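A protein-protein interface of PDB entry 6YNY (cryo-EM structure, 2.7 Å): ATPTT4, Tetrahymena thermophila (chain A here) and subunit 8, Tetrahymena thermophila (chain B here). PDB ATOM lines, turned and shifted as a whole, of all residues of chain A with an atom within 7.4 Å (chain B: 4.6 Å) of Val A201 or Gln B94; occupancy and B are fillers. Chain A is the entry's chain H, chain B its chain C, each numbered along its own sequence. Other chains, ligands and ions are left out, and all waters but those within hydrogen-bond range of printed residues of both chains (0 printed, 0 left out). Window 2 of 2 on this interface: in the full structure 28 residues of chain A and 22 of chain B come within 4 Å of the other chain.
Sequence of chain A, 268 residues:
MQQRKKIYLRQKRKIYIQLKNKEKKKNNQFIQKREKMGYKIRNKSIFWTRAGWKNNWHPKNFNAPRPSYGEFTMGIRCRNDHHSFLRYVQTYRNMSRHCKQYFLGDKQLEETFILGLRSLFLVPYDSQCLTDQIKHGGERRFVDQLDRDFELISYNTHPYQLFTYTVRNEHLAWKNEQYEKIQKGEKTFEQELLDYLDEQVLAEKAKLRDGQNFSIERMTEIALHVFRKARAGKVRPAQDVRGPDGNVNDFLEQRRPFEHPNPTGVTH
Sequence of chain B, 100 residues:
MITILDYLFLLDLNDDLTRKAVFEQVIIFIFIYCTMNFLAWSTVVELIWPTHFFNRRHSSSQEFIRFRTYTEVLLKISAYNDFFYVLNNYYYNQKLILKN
The side-chain amide nitrogen of Gln B94 is in hydrogen-bond range of the side-chain carboxylate of Asp A198 (3.3 Å).
The side-chain hydroxyl (OH) of Tyr B90 sits at hydrogen-bond distance from the backbone carbonyl oxygen (O) of Met A219, 3.0 Å away.
Among the printed residues, merely in contact across the chains: Leu A194 with Tyr B90 (3.8 Å), Leu A197 with Tyr B90 (3.7 Å), Val A201 with Tyr B90 (3.4 Å), Val A201 with Gln B94 (3.7 Å), Ile A216 with Tyr B91 (3.6 Å), Ile A216 with Lys B95 (3.7 Å), Met A219 with Gln B94 (3.3 Å) and Met A219 with Lys B95 (3.9 Å).
Printed residues of chain B within 4 Å of Val A201: Tyr B90 (3.4 Å) and Gln B94 (3.7 Å).
Of chain A, only Asp A198 (3.3 Å), Val A201 (3.7 Å) and Met A219 (3.3 Å) come within 4 Å of Gln B94.
Of the printed residues of chain A, Tyr B90 touches Leu A194 (3.8 Å), Leu A197 (3.7 Å), Val A201 (3.4 Å) and Met A219 (3.0 Å).
Of the printed residues of chain B, Ile A216 touches Tyr B91 and Lys B95.
Of the printed residues of chain B, Asp A198 touches Gln B94.
Of the printed residues of chain A, Lys B95 touches Ile A216 and Met A219.
Printed residues of chain B within 4 Å of Leu A197: Tyr B90 (3.7 Å).
Leu A202 touches none of the printed residues of chain B.
Lys A207 touches none of the printed residues of chain B.
The nearest printed residue of chain B that does not touch Val A201 is Leu B98 (7.3 Å).
The nearest residue of chain A that does not touch Gln B94 is Leu A197 (4.9 Å).
O of Leu A194 sits close to OD1 of Asp A198, at 2.7 Å.
The backbone NH (N) of Lys B99 is in hydrogen-bond range of the backbone carbonyl oxygen (O) of Gln B94, 2.8 Å away.
Of the 20 printed residues of chain A, 6 touch a printed residue of chain B.
Among the printed residues, 10 pairs touch across the chains.
Among the printed residues, no Asp or Glu carboxylate lies within 4 Å of a Lys or Arg side-chain nitrogen of the other chain.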
ATOM      1  N   LEU A 194      30.584 -15.029  -2.465  1.00  0.00           N
ATOM      2  CA  LEU A 194      29.669 -15.353  -1.378  1.00  0.00           C
ATOM      3  C   LEU A 194      28.770 -14.171  -1.052  1.00  0.00           C
ATOM      4  O   LEU A 194      27.571 -14.341  -0.805  1.00  0.00           O
ATOM      5  CB  LEU A 194      30.457 -15.777  -0.141  1.00  0.00           C
ATOM      6  CG  LEU A 194      31.226 -17.090  -0.245  1.00  0.00           C
ATOM      7  CD1 LEU A 194      32.199 -17.236   0.907  1.00  0.00           C
ATOM      8  CD2 LEU A 194      30.268 -18.256  -0.275  1.00  0.00           C
ATOM      9  N   ASP A 195      29.332 -12.962  -1.051  1.00  0.00           N
ATOM     10  CA  ASP A 195      28.525 -11.778  -0.793  1.00  0.00           C
ATOM     11  C   ASP A 195      27.643 -11.444  -1.988  1.00  0.00           C
ATOM     12  O   ASP A 195      26.499 -11.007  -1.822  1.00  0.00           O
ATOM     13  CB  ASP A 195      29.430 -10.598  -0.450  1.00  0.00           C
ATOM     14  CG  ASP A 195      30.318 -10.874   0.744  1.00  0.00           C
ATOM     15  OD1 ASP A 195      29.927 -11.696   1.600  1.00  0.00           O
ATOM     16  OD2 ASP A 195      31.406 -10.269   0.830  1.00  0.00           O
ATOM     17  N   TYR A 196      28.156 -11.646  -3.201  1.00  0.00           N
ATOM     18  CA  TYR A 196      27.363 -11.374  -4.391  1.00  0.00           C
ATOM     19  C   TYR A 196      26.249 -12.394  -4.563  1.00  0.00           C
ATOM     20  O   TYR A 196      25.228 -12.095  -5.192  1.00  0.00           O
ATOM     21  CB  TYR A 196      28.266 -11.356  -5.621  1.00  0.00           C
ATOM     22  CG  TYR A 196      27.554 -11.016  -6.905  1.00  0.00           C
ATOM     23  CD1 TYR A 196      27.293  -9.699  -7.247  1.00  0.00           C
ATOM     24  CD2 TYR A 196      27.153 -12.010  -7.780  1.00  0.00           C
ATOM     25  CE1 TYR A 196      26.646  -9.383  -8.421  1.00  0.00           C
ATOM     26  CE2 TYR A 196      26.505 -11.704  -8.956  1.00  0.00           C
ATOM     27  CZ  TYR A 196      26.256 -10.389  -9.271  1.00  0.00           C
ATOM     28  OH  TYR A 196      25.610 -10.082 -10.445  1.00  0.00           O
ATOM     29  N   LEU A 197      26.424 -13.598  -4.020  1.00  0.00           N
ATOM     30  CA  LEU A 197      25.384 -14.614  -4.111  1.00  0.00           C
ATOM     31  C   LEU A 197      24.318 -14.439  -3.040  1.00  0.00           C
ATOM     32  O   LEU A 197      23.144 -14.732  -3.289  1.00  0.00           O
ATOM     33  CB  LEU A 197      26.000 -16.006  -3.999  1.00  0.00           C
ATOM     34  CG  LEU A 197      26.871 -16.457  -5.167  1.00  0.00           C
ATOM     35  CD1 LEU A 197      27.565 -17.750  -4.825  1.00  0.00           C
ATOM     36  CD2 LEU A 197      26.038 -16.622  -6.415  1.00  0.00           C
ATOM     37  N   ASP A 198      24.699 -13.971  -1.853  1.00  0.00           N
ATOM     38  CA  ASP A 198      23.717 -13.764  -0.797  1.00  0.00           C
ATOM     39  C   ASP A 198      22.698 -12.706  -1.196  1.00  0.00           C
ATOM     40  O   ASP A 198      21.513 -12.817  -0.864  1.00  0.00           O
ATOM     41  CB  ASP A 198      24.417 -13.369   0.500  1.00  0.00           C
ATOM     42  CG  ASP A 198      25.321 -14.461   1.031  1.00  0.00           C
ATOM     43  OD1 ASP A 198      25.410 -15.527   0.385  1.00  0.00           O
ATOM     44  OD2 ASP A 198      25.943 -14.257   2.095  1.00  0.00           O
ATOM     45  N   GLU A 199      23.141 -11.670  -1.909  1.00  0.00           N
ATOM     46  CA  GLU A 199      22.226 -10.618  -2.331  1.00  0.00           C
ATOM     47  C   GLU A 199      21.352 -11.070  -3.494  1.00  0.00           C
ATOM     48  O   GLU A 199      20.179 -10.694  -3.574  1.00  0.00           O
ATOM     49  CB  GLU A 199      23.011  -9.364  -2.708  1.00  0.00           C
ATOM     50  CG  GLU A 199      23.940  -9.546  -3.886  1.00  0.00           C
ATOM     51  CD  GLU A 199      24.753  -8.302  -4.179  1.00  0.00           C
ATOM     52  OE1 GLU A 199      24.682  -7.345  -3.381  1.00  0.00           O
ATOM     53  OE2 GLU A 199      25.461  -8.278  -5.208  1.00  0.00           O
ATOM     54  N   GLN A 200      21.905 -11.875  -4.403  1.00  0.00           N
ATOM     55  CA  GLN A 200      21.111 -12.384  -5.514  1.00  0.00           C
ATOM     56  C   GLN A 200      19.975 -13.269  -5.025  1.00  0.00           C
ATOM     57  O   GLN A 200      18.927 -13.351  -5.675  1.00  0.00           O
ATOM     58  CB  GLN A 200      22.004 -13.153  -6.484  1.00  0.00           C
ATOM     59  CG  GLN A 200      22.943 -12.272  -7.287  1.00  0.00           C
ATOM     60  CD  GLN A 200      22.218 -11.354  -8.247  1.00  0.00           C
ATOM     61  OE1 GLN A 200      22.543 -10.171  -8.355  1.00  0.00           O
ATOM     62  NE2 GLN A 200      21.236 -11.894  -8.958  1.00  0.00           N
ATOM     63  N   VAL A 201      20.165 -13.940  -3.891  1.00  0.00           N
ATOM     64  CA  VAL A 201      19.103 -14.765  -3.327  1.00  0.00           C
ATOM     65  C   VAL A 201      17.995 -13.890  -2.760  1.00  0.00           C
ATOM     66  O   VAL A 201      16.805 -14.191  -2.913  1.00  0.00           O
ATOM     67  CB  VAL A 201      19.679 -15.714  -2.264  1.00  0.00           C
ATOM     68  CG1 VAL A 201      18.572 -16.449  -1.553  1.00  0.00           C
ATOM     69  CG2 VAL A 201      20.625 -16.695  -2.902  1.00  0.00           C
ATOM     70  N   LEU A 202      18.363 -12.795  -2.093  1.00  0.00           N
ATOM     71  CA  LEU A 202      17.359 -11.873  -1.578  1.00  0.00           C
ATOM     72  C   LEU A 202      16.523 -11.287  -2.706  1.00  0.00           C
ATOM     73  O   LEU A 202      15.302 -11.145  -2.577  1.00  0.00           O
ATOM     74  CB  LEU A 202      18.032 -10.756  -0.787  1.00  0.00           C
ATOM     75  CG  LEU A 202      18.817 -11.175   0.452  1.00  0.00           C
ATOM     76  CD1 LEU A 202      19.474  -9.965   1.084  1.00  0.00           C
ATOM     77  CD2 LEU A 202      17.916 -11.879   1.449  1.00  0.00           C
ATOM     78  N   ALA A 203      17.164 -10.946  -3.823  1.00  0.00           N
ATOM     79  CA  ALA A 203      16.429 -10.392  -4.952  1.00  0.00           C
ATOM     80  C   ALA A 203      15.437 -11.394  -5.523  1.00  0.00           C
ATOM     81  O   ALA A 203      14.365 -11.003  -5.997  1.00  0.00           O
ATOM     82  CB  ALA A 203      17.404  -9.944  -6.037  1.00  0.00           C
ATOM     83  N   GLU A 204      15.771 -12.684  -5.490  1.00  0.00           N
ATOM     84  CA  GLU A 204      14.884 -13.690  -6.060  1.00  0.00           C
ATOM     85  C   GLU A 204      13.722 -14.007  -5.131  1.00  0.00           C
ATOM     86  O   GLU A 204      12.582 -14.149  -5.589  1.00  0.00           O
ATOM     87  CB  GLU A 204      15.669 -14.960  -6.376  1.00  0.00           C
ATOM     88  CG  GLU A 204      16.627 -14.819  -7.542  1.00  0.00           C
ATOM     89  CD  GLU A 204      15.919 -14.574  -8.861  1.00  0.00           C
ATOM     90  OE1 GLU A 204      14.672 -14.631  -8.890  1.00  0.00           O
ATOM     91  OE2 GLU A 204      16.610 -14.323  -9.869  1.00  0.00           O
ATOM     92  N   LYS A 205      13.983 -14.122  -3.830  1.00  0.00           N
ATOM     93  CA  LYS A 205      12.916 -14.419  -2.885  1.00  0.00           C
ATOM     94  C   LYS A 205      12.112 -13.184  -2.513  1.00  0.00           C
ATOM     95  O   LYS A 205      11.000 -13.318  -1.991  1.00  0.00           O
ATOM     96  CB  LYS A 205      13.490 -15.065  -1.625  1.00  0.00           C
ATOM     97  CG  LYS A 205      14.281 -14.123  -0.746  1.00  0.00           C
ATOM     98  CD  LYS A 205      15.020 -14.880   0.348  1.00  0.00           C
ATOM     99  CE  LYS A 205      14.066 -15.657   1.237  1.00  0.00           C
ATOM    100  NZ  LYS A 205      14.759 -16.261   2.400  1.00  0.00           N
ATOM    101  N   ALA A 206      12.645 -11.988  -2.769  1.00  0.00           N
ATOM    102  CA  ALA A 206      11.868 -10.773  -2.572  1.00  0.00           C
ATOM    103  C   ALA A 206      10.784 -10.619  -3.629  1.00  0.00           C
ATOM    104  O   ALA A 206       9.800  -9.911  -3.393  1.00  0.00           O
ATOM    105  CB  ALA A 206      12.786  -9.553  -2.589  1.00  0.00           C
ATOM    106  N   LYS A 207      10.946 -11.265  -4.783  1.00  0.00           N
ATOM    107  CA  LYS A 207       9.930 -11.285  -5.825  1.00  0.00           C
ATOM    108  C   LYS A 207       9.173 -12.603  -5.878  1.00  0.00           C
ATOM    109  O   LYS A 207       8.128 -12.674  -6.534  1.00  0.00           O
ATOM    110  CB  LYS A 207      10.568 -11.021  -7.192  1.00  0.00           C
ATOM    111  CG  LYS A 207      11.599 -12.056  -7.602  1.00  0.00           C
ATOM    112  CD  LYS A 207      12.140 -11.790  -8.997  1.00  0.00           C
ATOM    113  CE  LYS A 207      12.985 -10.530  -9.041  1.00  0.00           C
ATOM    114  NZ  LYS A 207      13.606 -10.322 -10.378  1.00  0.00           N
ATOM    115  N   LEU A 208       9.672 -13.641  -5.208  1.00  0.00           N
ATOM    116  CA  LEU A 208       9.012 -14.944  -5.174  1.00  0.00           C
ATOM    117  C   LEU A 208       8.049 -14.957  -3.992  1.00  0.00           C
ATOM    118  O   LEU A 208       8.309 -15.538  -2.936  1.00  0.00           O
ATOM    119  CB  LEU A 208      10.042 -16.060  -5.069  1.00  0.00           C
ATOM    120  CG  LEU A 208       9.501 -17.488  -5.029  1.00  0.00           C
ATOM    121  CD1 LEU A 208       9.126 -17.958  -6.426  1.00  0.00           C
ATOM    122  CD2 LEU A 208      10.514 -18.419  -4.387  1.00  0.00           C
ATOM    123  N   PHE A 214      12.082 -22.004  -1.912  1.00  0.00           N
ATOM    124  CA  PHE A 214      13.334 -21.710  -2.608  1.00  0.00           C
ATOM    125  C   PHE A 214      14.176 -22.977  -2.593  1.00  0.00           C
ATOM    126  O   PHE A 214      14.975 -23.215  -1.687  1.00  0.00           O
ATOM    127  CB  PHE A 214      14.058 -20.541  -1.959  1.00  0.00           C
ATOM    128  CG  PHE A 214      14.960 -19.803  -2.899  1.00  0.00           C
ATOM    129  CD1 PHE A 214      14.433 -18.953  -3.852  1.00  0.00           C
ATOM    130  CD2 PHE A 214      16.330 -19.962  -2.836  1.00  0.00           C
ATOM    131  CE1 PHE A 214      15.254 -18.275  -4.723  1.00  0.00           C
ATOM    132  CE2 PHE A 214      17.155 -19.284  -3.707  1.00  0.00           C
ATOM    133  CZ  PHE A 214      16.616 -18.441  -4.651  1.00  0.00           C
ATOM    134  N   ILE A 216      16.814 -26.097  -3.532  1.00  0.00           N
ATOM    135  CA  ILE A 216      18.258 -26.147  -3.714  1.00  0.00           C
ATOM    136  C   ILE A 216      18.607 -26.089  -5.194  1.00  0.00           C
ATOM    137  O   ILE A 216      19.707 -25.660  -5.564  1.00  0.00           O
ATOM    138  CB  ILE A 216      18.828 -27.409  -3.041  1.00  0.00           C
ATOM    139  CG1 ILE A 216      20.353 -27.376  -3.015  1.00  0.00           C
ATOM    140  CG2 ILE A 216      18.359 -28.658  -3.749  1.00  0.00           C
ATOM    141  CD1 ILE A 216      20.910 -26.435  -1.992  1.00  0.00           C
ATOM    142  N   ARG A 218      17.143 -24.133  -7.499  1.00  0.00           N
ATOM    143  CA  ARG A 218      17.217 -22.719  -7.847  1.00  0.00           C
ATOM    144  C   ARG A 218      18.484 -22.090  -7.284  1.00  0.00           C
ATOM    145  O   ARG A 218      19.189 -21.353  -7.981  1.00  0.00           O
ATOM    146  CB  ARG A 218      15.977 -21.991  -7.334  1.00  0.00           C
ATOM    147  CG  ARG A 218      15.892 -20.539  -7.763  1.00  0.00           C
ATOM    148  CD  ARG A 218      15.428 -20.406  -9.197  1.00  0.00           C
ATOM    149  NE  ARG A 218      15.505 -19.026  -9.670  1.00  0.00           N
ATOM    150  CZ  ARG A 218      16.526 -18.515 -10.354  1.00  0.00           C
ATOM    151  NH1 ARG A 218      16.497 -17.245 -10.734  1.00  0.00           N
ATOM    152  NH2 ARG A 218      17.575 -19.264 -10.669  1.00  0.00           N
ATOM    153  N   MET A 219      18.792 -22.375  -6.016  1.00  0.00           N
ATOM    154  CA  MET A 219      20.019 -21.865  -5.422  1.00  0.00           C
ATOM    155  C   MET A 219      21.237 -22.274  -6.231  1.00  0.00           C
ATOM    156  O   MET A 219      22.215 -21.523  -6.312  1.00  0.00           O
ATOM    157  CB  MET A 219      20.153 -22.372  -3.991  1.00  0.00           C
ATOM    158  CG  MET A 219      19.089 -21.860  -3.053  1.00  0.00           C
ATOM    159  SD  MET A 219      19.110 -22.680  -1.449  1.00  0.00           S
ATOM    160  CE  MET A 219      20.776 -22.320  -0.903  1.00  0.00           C
ATOM    161  N   ILE A 222      21.633 -20.418  -9.764  1.00  0.00           N
ATOM    162  CA  ILE A 222      22.045 -19.034  -9.572  1.00  0.00           C
ATOM    163  C   ILE A 222      23.561 -18.947  -9.486  1.00  0.00           C
ATOM    164  O   ILE A 222      24.189 -18.084 -10.108  1.00  0.00           O
ATOM    165  CB  ILE A 222      21.381 -18.448  -8.315  1.00  0.00           C
ATOM    166  CG1 ILE A 222      19.883 -18.275  -8.542  1.00  0.00           C
ATOM    167  CG2 ILE A 222      22.023 -17.128  -7.948  1.00  0.00           C
ATOM    168  CD1 ILE A 222      19.123 -17.894  -7.304  1.00  0.00           C
ATOM    169  N   TYR B  90      28.257 -21.484   0.299  1.00  0.00           N
ATOM    170  CA  TYR B  90      27.017 -20.885  -0.179  1.00  0.00           C
ATOM    171  C   TYR B  90      25.815 -21.720   0.235  1.00  0.00           C
ATOM    172  O   TYR B  90      24.787 -21.178   0.656  1.00  0.00           O
ATOM    173  CB  TYR B  90      27.083 -20.723  -1.695  1.00  0.00           C
ATOM    174  CG  TYR B  90      25.784 -20.362  -2.370  1.00  0.00           C
ATOM    175  CD1 TYR B  90      25.163 -19.150  -2.126  1.00  0.00           C
ATOM    176  CD2 TYR B  90      25.195 -21.225  -3.279  1.00  0.00           C
ATOM    177  CE1 TYR B  90      23.985 -18.818  -2.752  1.00  0.00           C
ATOM    178  CE2 TYR B  90      24.021 -20.900  -3.908  1.00  0.00           C
ATOM    179  CZ  TYR B  90      23.420 -19.697  -3.644  1.00  0.00           C
ATOM    180  OH  TYR B  90      22.246 -19.381  -4.277  1.00  0.00           O
ATOM    181  N   TYR B  91      25.928 -23.043   0.130  1.00  0.00           N
ATOM    182  CA  TYR B  91      24.852 -23.914   0.583  1.00  0.00           C
ATOM    183  C   TYR B  91      24.722 -23.886   2.100  1.00  0.00           C
ATOM    184  O   TYR B  91      23.608 -23.900   2.633  1.00  0.00           O
ATOM    185  CB  TYR B  91      25.090 -25.341   0.097  1.00  0.00           C
ATOM    186  CG  TYR B  91      24.879 -25.571  -1.385  1.00  0.00           C
ATOM    187  CD1 TYR B  91      24.105 -24.712  -2.144  1.00  0.00           C
ATOM    188  CD2 TYR B  91      25.446 -26.665  -2.020  1.00  0.00           C
ATOM    189  CE1 TYR B  91      23.907 -24.931  -3.488  1.00  0.00           C
ATOM    190  CE2 TYR B  91      25.254 -26.889  -3.364  1.00  0.00           C
ATOM    191  CZ  TYR B  91      24.484 -26.019  -4.094  1.00  0.00           C
ATOM    192  OH  TYR B  91      24.287 -26.237  -5.434  1.00  0.00           O
ATOM    193  N   TYR B  92      25.847 -23.854   2.812  1.00  0.00           N
ATOM    194  CA  TYR B  92      25.800 -23.880   4.268  1.00  0.00           C
ATOM    195  C   TYR B  92      25.152 -22.618   4.820  1.00  0.00           C
ATOM    196  O   TYR B  92      24.222 -22.690   5.631  1.00  0.00           O
ATOM    197  CB  TYR B  92      27.205 -24.042   4.838  1.00  0.00           C
ATOM    198  CG  TYR B  92      27.844 -25.389   4.605  1.00  0.00           C
ATOM    199  CD1 TYR B  92      27.228 -26.355   3.828  1.00  0.00           C
ATOM    200  CD2 TYR B  92      29.065 -25.697   5.178  1.00  0.00           C
ATOM    201  CE1 TYR B  92      27.815 -27.580   3.623  1.00  0.00           C
ATOM    202  CE2 TYR B  92      29.655 -26.919   4.979  1.00  0.00           C
ATOM    203  CZ  TYR B  92      29.028 -27.856   4.203  1.00  0.00           C
ATOM    204  OH  TYR B  92      29.621 -29.076   4.006  1.00  0.00           O
ATOM    205  N   ASN B  93      25.637 -21.451   4.397  1.00  0.00           N
ATOM    206  CA  ASN B  93      25.134 -20.200   4.950  1.00  0.00           C
ATOM    207  C   ASN B  93      23.648 -20.024   4.683  1.00  0.00           C
ATOM    208  O   ASN B  93      22.927 -19.472   5.521  1.00  0.00           O
ATOM    209  CB  ASN B  93      25.912 -19.022   4.371  1.00  0.00           C
ATOM    210  CG  ASN B  93      27.402 -19.144   4.590  1.00  0.00           C
ATOM    211  OD1 ASN B  93      27.852 -19.711   5.584  1.00  0.00           O
ATOM    212  ND2 ASN B  93      28.180 -18.610   3.659  1.00  0.00           N
ATOM    213  N   GLN B  94      23.169 -20.487   3.530  1.00  0.00           N
ATOM    214  CA  GLN B  94      21.777 -20.265   3.164  1.00  0.00           C
ATOM    215  C   GLN B  94      20.836 -21.208   3.900  1.00  0.00           C
ATOM    216  O   GLN B  94      19.766 -20.787   4.351  1.00  0.00           O
ATOM    217  CB  GLN B  94      21.602 -20.424   1.656  1.00  0.00           C
ATOM    218  CG  GLN B  94      22.267 -19.343   0.844  1.00  0.00           C
ATOM    219  CD  GLN B  94      21.650 -17.984   1.073  1.00  0.00           C
ATOM    220  OE1 GLN B  94      20.454 -17.868   1.330  1.00  0.00           O
ATOM    221  NE2 GLN B  94      22.468 -16.944   0.988  1.00  0.00           N
ATOM    222  N   LYS B  95      21.209 -22.476   4.033  1.00  0.00           N
ATOM    223  CA  LYS B  95      20.318 -23.493   4.575  1.00  0.00           C
ATOM    224  C   LYS B  95      20.599 -23.832   6.030  1.00  0.00           C
ATOM    225  O   LYS B  95      19.657 -24.009   6.807  1.00  0.00           O
ATOM    226  CB  LYS B  95      20.408 -24.764   3.732  1.00  0.00           C
ATOM    227  CG  LYS B  95      20.126 -24.528   2.269  1.00  0.00           C
ATOM    228  CD  LYS B  95      20.007 -25.823   1.508  1.00  0.00           C
ATOM    229  CE  LYS B  95      18.665 -26.492   1.740  1.00  0.00           C
ATOM    230  NZ  LYS B  95      17.541 -25.671   1.220  1.00  0.00           N
ATOM    231  N   LEU B  96      21.866 -23.933   6.421  1.00  0.00           N
ATOM    232  CA  LEU B  96      22.184 -24.308   7.793  1.00  0.00           C
ATOM    233  C   LEU B  96      22.178 -23.111   8.730  1.00  0.00           C
ATOM    234  O   LEU B  96      21.951 -23.273   9.933  1.00  0.00           O
ATOM    235  CB  LEU B  96      23.546 -24.995   7.853  1.00  0.00           C
ATOM    236  CG  LEU B  96      23.764 -26.153   6.887  1.00  0.00           C
ATOM    237  CD1 LEU B  96      25.125 -26.756   7.126  1.00  0.00           C
ATOM    238  CD2 LEU B  96      22.686 -27.194   7.034  1.00  0.00           C
ATOM    239  N   LEU B  98      21.070 -19.371   7.547  1.00  0.00           N
ATOM    240  CA  LEU B  98      19.959 -18.491   7.218  1.00  0.00           C
ATOM    241  C   LEU B  98      18.676 -19.242   6.892  1.00  0.00           C
ATOM    242  O   LEU B  98      17.667 -18.603   6.577  1.00  0.00           O
ATOM    243  CB  LEU B  98      20.334 -17.595   6.035  1.00  0.00           C
ATOM    244  CG  LEU B  98      21.577 -16.728   6.229  1.00  0.00           C
ATOM    245  CD1 LEU B  98      21.922 -16.012   4.942  1.00  0.00           C
ATOM    246  CD2 LEU B  98      21.373 -15.735   7.353  1.00  0.00           C
ATOM    247  N   LYS B  99      18.685 -20.567   6.963  1.00  0.00           N
ATOM    248  CA  LYS B  99      17.518 -21.362   6.606  1.00  0.00           C
ATOM    249  C   LYS B  99      17.015 -21.007   5.210  1.00  0.00           C
ATOM    250  O   LYS B  99      16.137 -20.161   5.053  1.00  0.00           O
ATOM    251  CB  LYS B  99      16.402 -21.168   7.627  1.00  0.00           C
ATOM    252  CG  LYS B  99      16.498 -22.086   8.832  1.00  0.00           C
ATOM    253  CD  LYS B  99      17.761 -21.850   9.631  1.00  0.00           C
ATOM    254  CE  LYS B  99      17.784 -22.721  10.872  1.00  0.00           C
ATOM    255  NZ  LYS B  99      18.993 -22.501  11.698  1.00  0.00           N
